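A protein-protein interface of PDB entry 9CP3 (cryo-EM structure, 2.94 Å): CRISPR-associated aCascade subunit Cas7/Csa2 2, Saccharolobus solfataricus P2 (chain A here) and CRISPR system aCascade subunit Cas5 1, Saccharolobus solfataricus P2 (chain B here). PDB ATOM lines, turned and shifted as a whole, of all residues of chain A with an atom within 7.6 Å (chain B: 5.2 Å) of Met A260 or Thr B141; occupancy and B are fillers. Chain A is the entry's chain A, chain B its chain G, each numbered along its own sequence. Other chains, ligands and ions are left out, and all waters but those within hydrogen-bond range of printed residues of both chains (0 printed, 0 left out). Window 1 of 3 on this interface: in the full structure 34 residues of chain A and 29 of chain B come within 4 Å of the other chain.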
ATOM      1  N   ILE A   2       0.451  17.844   1.107  1.00  0.00           N
ATOM      2  CA  ILE A   2       1.523  18.500   1.843  1.00  0.00           C
ATOM      3  C   ILE A   2       2.391  19.262   0.854  1.00  0.00           C
ATOM      4  O   ILE A   2       2.693  18.761  -0.234  1.00  0.00           O
ATOM      5  CB  ILE A   2       2.362  17.479   2.641  1.00  0.00           C
ATOM      6  CG1 ILE A   2       1.490  16.772   3.678  1.00  0.00           C
ATOM      7  CG2 ILE A   2       3.547  18.156   3.309  1.00  0.00           C
ATOM      8  CD1 ILE A   2       1.965  15.385   4.032  1.00  0.00           C
ATOM      9  N   SER A   3       2.775  20.481   1.215  1.00  0.00           N
ATOM     10  CA  SER A   3       3.655  21.282   0.378  1.00  0.00           C
ATOM     11  C   SER A   3       4.740  21.903   1.242  1.00  0.00           C
ATOM     12  O   SER A   3       4.548  22.109   2.441  1.00  0.00           O
ATOM     13  CB  SER A   3       2.882  22.372  -0.362  1.00  0.00           C
ATOM     14  OG  SER A   3       1.756  21.831  -1.029  1.00  0.00           O
ATOM     15  N   GLY A   4       5.877  22.208   0.632  1.00  0.00           N
ATOM     16  CA  GLY A   4       6.988  22.764   1.385  1.00  0.00           C
ATOM     17  C   GLY A   4       7.906  23.602   0.527  1.00  0.00           C
ATOM     18  O   GLY A   4       8.037  23.382  -0.681  1.00  0.00           O
ATOM     19  N   SER A   5       8.547  24.578   1.170  1.00  0.00           N
ATOM     20  CA  SER A   5       9.571  25.416   0.561  1.00  0.00           C
ATOM     21  C   SER A   5      10.704  25.595   1.559  1.00  0.00           C
ATOM     22  O   SER A   5      10.465  25.971   2.712  1.00  0.00           O
ATOM     23  CB  SER A   5       9.005  26.777   0.145  1.00  0.00           C
ATOM     24  OG  SER A   5       9.929  27.488  -0.659  1.00  0.00           O
ATOM     25  N   LYS A 138       6.755  15.552  -5.872  1.00  0.00           N
ATOM     26  CA  LYS A 138       7.197  16.455  -6.923  1.00  0.00           C
ATOM     27  C   LYS A 138       8.274  17.371  -6.362  1.00  0.00           C
ATOM     28  O   LYS A 138       8.053  18.046  -5.351  1.00  0.00           O
ATOM     29  CB  LYS A 138       6.027  17.271  -7.473  1.00  0.00           C
ATOM     30  CG  LYS A 138       4.803  16.436  -7.807  1.00  0.00           C
ATOM     31  CD  LYS A 138       3.553  17.290  -7.874  1.00  0.00           C
ATOM     32  CE  LYS A 138       2.410  16.533  -8.525  1.00  0.00           C
ATOM     33  NZ  LYS A 138       1.944  15.392  -7.689  1.00  0.00           N
ATOM     34  N   SER A 187      11.557  23.810  -3.539  1.00  0.00           N
ATOM     35  CA  SER A 187      10.218  23.538  -3.039  1.00  0.00           C
ATOM     36  C   SER A 187       9.749  22.180  -3.545  1.00  0.00           C
ATOM     37  O   SER A 187      10.245  21.662  -4.550  1.00  0.00           O
ATOM     38  CB  SER A 187       9.228  24.628  -3.464  1.00  0.00           C
ATOM     39  OG  SER A 187       9.134  24.703  -4.876  1.00  0.00           O
ATOM     40  N   PHE A 188       8.773  21.611  -2.842  1.00  0.00           N
ATOM     41  CA  PHE A 188       8.292  20.274  -3.161  1.00  0.00           C
ATOM     42  C   PHE A 188       6.833  20.121  -2.757  1.00  0.00           C
ATOM     43  O   PHE A 188       6.300  20.888  -1.950  1.00  0.00           O
ATOM     44  CB  PHE A 188       9.145  19.196  -2.477  1.00  0.00           C
ATOM     45  CG  PHE A 188       8.994  19.155  -0.981  1.00  0.00           C
ATOM     46  CD1 PHE A 188       8.004  18.387  -0.387  1.00  0.00           C
ATOM     47  CD2 PHE A 188       9.851  19.874  -0.168  1.00  0.00           C
ATOM     48  CE1 PHE A 188       7.869  18.349   0.984  1.00  0.00           C
ATOM     49  CE2 PHE A 188       9.720  19.837   1.204  1.00  0.00           C
ATOM     50  CZ  PHE A 188       8.728  19.073   1.780  1.00  0.00           C
ATOM     51  N   GLU A 189       6.200  19.099  -3.334  1.00  0.00           N
ATOM     52  CA  GLU A 189       4.833  18.722  -3.002  1.00  0.00           C
ATOM     53  C   GLU A 189       4.756  17.212  -2.810  1.00  0.00           C
ATOM     54  O   GLU A 189       5.467  16.450  -3.468  1.00  0.00           O
ATOM     55  CB  GLU A 189       3.841  19.169  -4.091  1.00  0.00           C
ATOM     56  CG  GLU A 189       2.387  18.804  -3.806  1.00  0.00           C
ATOM     57  CD  GLU A 189       1.444  19.212  -4.919  1.00  0.00           C
ATOM     58  OE1 GLU A 189       1.905  19.865  -5.879  1.00  0.00           O
ATOM     59  OE2 GLU A 189       0.242  18.880  -4.835  1.00  0.00           O
ATOM     60  N   LEU A 190       3.877  16.783  -1.906  1.00  0.00           N
ATOM     61  CA  LEU A 190       3.649  15.370  -1.631  1.00  0.00           C
ATOM     62  C   LEU A 190       2.152  15.157  -1.483  1.00  0.00           C
ATOM     63  O   LEU A 190       1.531  15.725  -0.579  1.00  0.00           O
ATOM     64  CB  LEU A 190       4.393  14.925  -0.367  1.00  0.00           C
ATOM     65  CG  LEU A 190       4.250  13.470   0.083  1.00  0.00           C
ATOM     66  CD1 LEU A 190       5.577  12.946   0.598  1.00  0.00           C
ATOM     67  CD2 LEU A 190       3.186  13.335   1.159  1.00  0.00           C
ATOM     68  N   THR A 253       3.044  23.446   4.495  1.00  0.00           N
ATOM     69  CA  THR A 253       1.602  23.569   4.643  1.00  0.00           C
ATOM     70  C   THR A 253       0.955  22.200   4.483  1.00  0.00           C
ATOM     71  O   THR A 253       1.205  21.499   3.493  1.00  0.00           O
ATOM     72  CB  THR A 253       1.022  24.543   3.617  1.00  0.00           C
ATOM     73  OG1 THR A 253       1.205  24.012   2.297  1.00  0.00           O
ATOM     74  CG2 THR A 253       1.707  25.895   3.718  1.00  0.00           C
ATOM     75  N   THR A 255      -2.673  20.672   4.004  1.00  0.00           N
ATOM     76  CA  THR A 255      -4.002  21.097   3.582  1.00  0.00           C
ATOM     77  C   THR A 255      -4.836  19.909   3.120  1.00  0.00           C
ATOM     78  O   THR A 255      -4.404  18.757   3.225  1.00  0.00           O
ATOM     79  CB  THR A 255      -3.922  22.125   2.448  1.00  0.00           C
ATOM     80  OG1 THR A 255      -3.599  21.461   1.221  1.00  0.00           O
ATOM     81  CG2 THR A 255      -2.874  23.189   2.741  1.00  0.00           C
ATOM     82  N   PHE A 257      -6.840  20.662   0.062  1.00  0.00           N
ATOM     83  CA  PHE A 257      -7.125  21.151  -1.276  1.00  0.00           C
ATOM     84  C   PHE A 257      -5.805  21.469  -1.958  1.00  0.00           C
ATOM     85  O   PHE A 257      -4.785  21.660  -1.287  1.00  0.00           O
ATOM     86  CB  PHE A 257      -8.018  22.401  -1.235  1.00  0.00           C
ATOM     87  CG  PHE A 257      -7.557  23.446  -0.259  1.00  0.00           C
ATOM     88  CD1 PHE A 257      -6.601  24.378  -0.622  1.00  0.00           C
ATOM     89  CD2 PHE A 257      -8.081  23.496   1.020  1.00  0.00           C
ATOM     90  CE1 PHE A 257      -6.176  25.337   0.272  1.00  0.00           C
ATOM     91  CE2 PHE A 257      -7.659  24.452   1.918  1.00  0.00           C
ATOM     92  CZ  PHE A 257      -6.705  25.374   1.544  1.00  0.00           C
ATOM     93  N   PRO A 258      -5.779  21.504  -3.291  1.00  0.00           N
ATOM     94  CA  PRO A 258      -4.528  21.826  -3.989  1.00  0.00           C
ATOM     95  C   PRO A 258      -3.995  23.191  -3.576  1.00  0.00           C
ATOM     96  O   PRO A 258      -4.750  24.155  -3.431  1.00  0.00           O
ATOM     97  CB  PRO A 258      -4.930  21.799  -5.466  1.00  0.00           C
ATOM     98  CG  PRO A 258      -6.108  20.896  -5.514  1.00  0.00           C
ATOM     99  CD  PRO A 258      -6.847  21.114  -4.228  1.00  0.00           C
ATOM    100  N   PHE A 259      -2.679  23.265  -3.397  1.00  0.00           N
ATOM    101  CA  PHE A 259      -2.035  24.479  -2.910  1.00  0.00           C
ATOM    102  C   PHE A 259      -0.533  24.377  -3.128  1.00  0.00           C
ATOM    103  O   PHE A 259       0.042  23.287  -3.071  1.00  0.00           O
ATOM    104  CB  PHE A 259      -2.336  24.714  -1.425  1.00  0.00           C
ATOM    105  CG  PHE A 259      -1.937  26.071  -0.938  1.00  0.00           C
ATOM    106  CD1 PHE A 259      -2.367  27.209  -1.595  1.00  0.00           C
ATOM    107  CD2 PHE A 259      -1.123  26.209   0.171  1.00  0.00           C
ATOM    108  CE1 PHE A 259      -1.999  28.459  -1.151  1.00  0.00           C
ATOM    109  CE2 PHE A 259      -0.751  27.457   0.621  1.00  0.00           C
ATOM    110  CZ  PHE A 259      -1.187  28.584  -0.043  1.00  0.00           C
ATOM    111  N   MET A 260       0.092  25.531  -3.372  1.00  0.00           N
ATOM    112  CA  MET A 260       1.537  25.640  -3.528  1.00  0.00           C
ATOM    113  C   MET A 260       2.035  26.944  -2.914  1.00  0.00           C
ATOM    114  O   MET A 260       1.610  28.027  -3.334  1.00  0.00           O
ATOM    115  CB  MET A 260       1.931  25.570  -5.004  1.00  0.00           C
ATOM    116  CG  MET A 260       1.901  24.177  -5.599  1.00  0.00           C
ATOM    117  SD  MET A 260       3.194  23.120  -4.927  1.00  0.00           S
ATOM    118  CE  MET A 260       4.652  24.049  -5.385  1.00  0.00           C
ATOM    119  N   PRO A 261       2.922  26.888  -1.924  1.00  0.00           N
ATOM    120  CA  PRO A 261       3.408  28.123  -1.300  1.00  0.00           C
ATOM    121  C   PRO A 261       4.326  28.899  -2.231  1.00  0.00           C
ATOM    122  O   PRO A 261       4.810  28.394  -3.246  1.00  0.00           O
ATOM    123  CB  PRO A 261       4.162  27.631  -0.060  1.00  0.00           C
ATOM    124  CG  PRO A 261       4.511  26.226  -0.352  1.00  0.00           C
ATOM    125  CD  PRO A 261       3.480  25.684  -1.291  1.00  0.00           C
ATOM    126  N   GLU A 262       4.551  30.159  -1.871  1.00  0.00           N
ATOM    127  CA  GLU A 262       5.403  31.024  -2.668  1.00  0.00           C
ATOM    128  C   GLU A 262       6.861  30.578  -2.584  1.00  0.00           C
ATOM    129  O   GLU A 262       7.293  30.017  -1.573  1.00  0.00           O
ATOM    130  CB  GLU A 262       5.283  32.470  -2.202  1.00  0.00           C
ATOM    131  CG  GLU A 262       3.872  33.006  -2.235  1.00  0.00           C
ATOM    132  CD  GLU A 262       3.825  34.499  -2.463  1.00  0.00           C
ATOM    133  OE1 GLU A 262       4.770  35.197  -2.042  1.00  0.00           O
ATOM    134  OE2 GLU A 262       2.841  34.977  -3.066  1.00  0.00           O
ATOM    135  N   PRO A 263       7.642  30.821  -3.635  1.00  0.00           N
ATOM    136  CA  PRO A 263       9.068  30.486  -3.585  1.00  0.00           C
ATOM    137  C   PRO A 263       9.808  31.356  -2.584  1.00  0.00           C
ATOM    138  O   PRO A 263       9.411  32.485  -2.289  1.00  0.00           O
ATOM    139  CB  PRO A 263       9.546  30.753  -5.018  1.00  0.00           C
ATOM    140  CG  PRO A 263       8.575  31.741  -5.558  1.00  0.00           C
ATOM    141  CD  PRO A 263       7.255  31.405  -4.930  1.00  0.00           C
ATOM    142  N   THR A 273       2.602  33.901   1.849  1.00  0.00           N
ATOM    143  CA  THR A 273       2.004  32.590   1.642  1.00  0.00           C
ATOM    144  C   THR A 273       0.934  32.299   2.687  1.00  0.00           C
ATOM    145  O   THR A 273      -0.051  31.627   2.380  1.00  0.00           O
ATOM    146  CB  THR A 273       3.074  31.493   1.622  1.00  0.00           C
ATOM    147  OG1 THR A 273       2.517  30.299   1.059  1.00  0.00           O
ATOM    148  CG2 THR A 273       3.584  31.182   3.014  1.00  0.00           C
ATOM    149  N   ARG A 276      -2.179  34.239   1.351  1.00  0.00           N
ATOM    150  CA  ARG A 276      -2.816  33.589   0.209  1.00  0.00           C
ATOM    151  C   ARG A 276      -3.355  32.209   0.567  1.00  0.00           C
ATOM    152  O   ARG A 276      -4.329  31.759  -0.041  1.00  0.00           O
ATOM    153  CB  ARG A 276      -1.852  33.506  -0.973  1.00  0.00           C
ATOM    154  CG  ARG A 276      -0.624  32.669  -0.728  1.00  0.00           C
ATOM    155  CD  ARG A 276       0.393  32.883  -1.829  1.00  0.00           C
ATOM    156  NE  ARG A 276       0.027  32.181  -3.053  1.00  0.00           N
ATOM    157  CZ  ARG A 276       0.419  30.950  -3.353  1.00  0.00           C
ATOM    158  NH1 ARG A 276       1.195  30.255  -2.538  1.00  0.00           N
ATOM    159  NH2 ARG A 276       0.019  30.403  -4.496  1.00  0.00           N
ATOM    160  N   LEU A 277      -2.768  31.534   1.559  1.00  0.00           N
ATOM    161  CA  LEU A 277      -3.360  30.300   2.063  1.00  0.00           C
ATOM    162  C   LEU A 277      -4.711  30.560   2.709  1.00  0.00           C
ATOM    163  O   LEU A 277      -5.669  29.811   2.485  1.00  0.00           O
ATOM    164  CB  LEU A 277      -2.415  29.639   3.068  1.00  0.00           C
ATOM    165  CG  LEU A 277      -3.042  28.629   4.034  1.00  0.00           C
ATOM    166  CD1 LEU A 277      -3.356  27.325   3.322  1.00  0.00           C
ATOM    167  CD2 LEU A 277      -2.140  28.386   5.237  1.00  0.00           C
ATOM    168  N   HIS B  11       8.613  29.339  -9.323  1.00  0.00           N
ATOM    169  CA  HIS B  11       9.765  29.128  -8.451  1.00  0.00           C
ATOM    170  C   HIS B  11      11.075  29.166  -9.232  1.00  0.00           C
ATOM    171  O   HIS B  11      11.995  29.911  -8.878  1.00  0.00           O
ATOM    172  CB  HIS B  11       9.621  27.800  -7.707  1.00  0.00           C
ATOM    173  CG  HIS B  11       8.360  27.688  -6.910  1.00  0.00           C
ATOM    174  ND1 HIS B  11       8.355  27.637  -5.533  1.00  0.00           N
ATOM    175  CD2 HIS B  11       7.065  27.613  -7.294  1.00  0.00           C
ATOM    176  CE1 HIS B  11       7.109  27.538  -5.103  1.00  0.00           C
ATOM    177  NE2 HIS B  11       6.307  27.522  -6.152  1.00  0.00           N
ATOM    178  N   ALA B  39      -3.474  22.647 -16.628  1.00  0.00           N
ATOM    179  CA  ALA B  39      -3.325  23.173 -15.277  1.00  0.00           C
ATOM    180  C   ALA B  39      -4.676  23.485 -14.648  1.00  0.00           C
ATOM    181  O   ALA B  39      -4.845  23.333 -13.434  1.00  0.00           O
ATOM    182  CB  ALA B  39      -2.443  24.419 -15.291  1.00  0.00           C
ATOM    183  N   TYR B  42      -6.469  20.130 -13.759  1.00  0.00           N
ATOM    184  CA  TYR B  42      -5.936  19.484 -12.562  1.00  0.00           C
ATOM    185  C   TYR B  42      -6.861  19.661 -11.365  1.00  0.00           C
ATOM    186  O   TYR B  42      -6.914  18.790 -10.489  1.00  0.00           O
ATOM    187  CB  TYR B  42      -4.543  20.033 -12.242  1.00  0.00           C
ATOM    188  CG  TYR B  42      -4.012  19.651 -10.872  1.00  0.00           C
ATOM    189  CD1 TYR B  42      -4.277  20.434  -9.755  1.00  0.00           C
ATOM    190  CD2 TYR B  42      -3.247  18.508 -10.699  1.00  0.00           C
ATOM    191  CE1 TYR B  42      -3.796  20.089  -8.509  1.00  0.00           C
ATOM    192  CE2 TYR B  42      -2.760  18.157  -9.455  1.00  0.00           C
ATOM    193  CZ  TYR B  42      -3.039  18.951  -8.364  1.00  0.00           C
ATOM    194  OH  TYR B  42      -2.557  18.605  -7.123  1.00  0.00           O
ATOM    195  N   SER B 139      -6.732  26.902  -7.609  1.00  0.00           N
ATOM    196  CA  SER B 139      -5.932  25.690  -7.452  1.00  0.00           C
ATOM    197  C   SER B 139      -5.256  25.396  -8.788  1.00  0.00           C
ATOM    198  O   SER B 139      -5.750  24.601  -9.592  1.00  0.00           O
ATOM    199  CB  SER B 139      -6.808  24.525  -6.980  1.00  0.00           C
ATOM    200  OG  SER B 139      -7.907  24.327  -7.853  1.00  0.00           O
ATOM    201  N   ILE B 140      -4.117  26.041  -9.021  1.00  0.00           N
ATOM    202  CA  ILE B 140      -3.313  25.831 -10.218  1.00  0.00           C
ATOM    203  C   ILE B 140      -1.917  25.435  -9.767  1.00  0.00           C
ATOM    204  O   ILE B 140      -1.262  26.182  -9.029  1.00  0.00           O
ATOM    205  CB  ILE B 140      -3.270  27.079 -11.113  1.00  0.00           C
ATOM    206  CG1 ILE B 140      -4.628  27.305 -11.781  1.00  0.00           C
ATOM    207  CG2 ILE B 140      -2.181  26.945 -12.163  1.00  0.00           C
ATOM    208  CD1 ILE B 140      -4.730  28.617 -12.527  1.00  0.00           C
ATOM    209  N   THR B 141      -1.467  24.260 -10.199  1.00  0.00           N
ATOM    210  CA  THR B 141      -0.147  23.758  -9.849  1.00  0.00           C
ATOM    211  C   THR B 141       0.499  23.132 -11.075  1.00  0.00           C
ATOM    212  O   THR B 141      -0.186  22.644 -11.977  1.00  0.00           O
ATOM    213  CB  THR B 141      -0.201  22.709  -8.723  1.00  0.00           C
ATOM    214  OG1 THR B 141      -0.813  21.510  -9.213  1.00  0.00           O
ATOM    215  CG2 THR B 141      -0.987  23.222  -7.523  1.00  0.00           C
ATOM    216  N   ARG B 142       1.832  23.153 -11.090  1.00  0.00           N
ATOM    217  CA  ARG B 142       2.643  22.358 -12.011  1.00  0.00           C
ATOM    218  C   ARG B 142       2.314  22.694 -13.470  1.00  0.00           C
ATOM    219  O   ARG B 142       1.798  21.878 -14.232  1.00  0.00           O
ATOM    220  CB  ARG B 142       2.456  20.861 -11.735  1.00  0.00           C
ATOM    221  CG  ARG B 142       3.455  19.972 -12.452  1.00  0.00           C
ATOM    222  CD  ARG B 142       3.312  18.518 -12.042  1.00  0.00           C
ATOM    223  NE  ARG B 142       2.005  17.967 -12.374  1.00  0.00           N
ATOM    224  CZ  ARG B 142       1.693  17.453 -13.556  1.00  0.00           C
ATOM    225  NH1 ARG B 142       2.566  17.421 -14.548  1.00  0.00           N
ATOM    226  NH2 ARG B 142       0.477  16.949 -13.742  1.00  0.00           N
ATOM    227  N   ILE B 143       2.626  23.933 -13.842  1.00  0.00           N
ATOM    228  CA  ILE B 143       2.491  24.332 -15.240  1.00  0.00           C
ATOM    229  C   ILE B 143       3.628  23.675 -16.018  1.00  0.00           C
ATOM    230  O   ILE B 143       4.800  24.007 -15.825  1.00  0.00           O
ATOM    231  CB  ILE B 143       2.503  25.856 -15.401  1.00  0.00           C
ATOM    232  CG1 ILE B 143       1.107  26.427 -15.149  1.00  0.00           C
ATOM    233  CG2 ILE B 143       2.952  26.254 -16.799  1.00  0.00           C
ATOM    234  CD1 ILE B 143       1.049  27.934 -15.212  1.00  0.00           C
ATOM    235  N   LEU B 149       7.188  23.555 -11.374  1.00  0.00           N
ATOM    236  CA  LEU B 149       6.189  23.966 -10.399  1.00  0.00           C
ATOM    237  C   LEU B 149       5.724  25.391 -10.673  1.00  0.00           C
ATOM    238  O   LEU B 149       6.518  26.262 -11.038  1.00  0.00           O
ATOM    239  CB  LEU B 149       6.754  23.863  -8.983  1.00  0.00           C
ATOM    240  CG  LEU B 149       6.903  22.451  -8.418  1.00  0.00           C
ATOM    241  CD1 LEU B 149       7.582  22.489  -7.060  1.00  0.00           C
ATOM    242  CD2 LEU B 149       5.546  21.775  -8.323  1.00  0.00           C
ATOM    243  N   ALA B 150       4.428  25.624 -10.502  1.00  0.00           N
ATOM    244  CA  ALA B 150       3.819  26.933 -10.686  1.00  0.00           C
ATOM    245  C   ALA B 150       3.174  27.384  -9.377  1.00  0.00           C
ATOM    246  O   ALA B 150       3.245  26.699  -8.355  1.00  0.00           O
ATOM    247  CB  ALA B 150       2.799  26.904 -11.826  1.00  0.00           C
ATOM    248  N   SER B 151       2.538  28.553  -9.412  1.00  0.00           N
ATOM    249  CA  SER B 151       1.868  29.080  -8.230  1.00  0.00           C
ATOM    250  C   SER B 151       0.787  30.061  -8.660  1.00  0.00           C
ATOM    251  O   SER B 151       0.792  30.562  -9.786  1.00  0.00           O
ATOM    252  CB  SER B 151       2.861  29.761  -7.282  1.00  0.00           C
ATOM    253  OG  SER B 151       3.737  28.815  -6.696  1.00  0.00           O
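Of chain A, only Met A260 comes within 4 Å of Thr B141.
Of the printed residues of chain A, Ala B150 touches Met A260.
Of the printed residues of chain A, Leu B149 touches Ser A187 and Met A260.
Of the printed residues of chain A, Ser B151 touches Pro A261.
Of the printed residues of chain B, Pro A261 touches His B11 and Ser B151.
Of the printed residues of chain B, Ser A187 touches His B11 (3.1 Å) and Leu B149 (3.5 Å).
Thr A253 touches none of the printed residues of chain B.
Arg B142 touches none of the printed residues of chain A.
The nearest residue of chain A that does not touch Thr B141 is Phe A259 (4.5 Å).
The nearest printed residue of chain B that does not touch Pro A263 is Ser B151 (4.7 Å).
The guanidinium group (NE) of Arg A276 is in salt-bridge range of the side-chain carboxylate (OE2) of Glu A262, 3.97 Å away.
N of Lys A138 is in hydrogen-bond range of O of Glu A189 (2.9 Å).
NE2 of His B11 sits at hydrogen-bond distance from OG of Ser B151 (2.9 Å).
The guanidinium group (NH1) of Arg A276 lies within hydrogen-bond range of the backbone carbonyl oxygen (O) of Met A260, 2.4 Å away.
Of the 21 printed residues of chain A, 7 touch a printed residue of chain B.
Hydrophobic or aromatic side chains of chain A that line the printed part of chain B: Pro A258, Met A260 and Pro A263.
Of the 11 printed residues of chain B, 7 touch a printed residue of chain A.
NE2 of His B11 sits close to O of Pro A261.
OG of Ser A187 is in hydrogen-bond range of ND1 of His B11, at 3.1 Å.
Ser A187 touches Leu B149 (OG to CD1, 3.5 Å).
Pro A258 touches Tyr B42 (CB to CE1, 3.7 Å).
Pro A258 touches Ser B139.
His B11 touches Met A260 (NE2 to CE, 3.9 Å).
Thr B141 touches Met A260 (CG2 to CG, 3.6 Å).
Met A260 touches Leu B149.
Met A260 touches Ala B150.
Pro A261 touches Ser B151 (O to OG, 3.6 Å).
C of Glu A262 touches CE1 of His B11, at 3.96 Å.
Pro A263 touches His B11 (CB to ND1, 3.4 Å).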
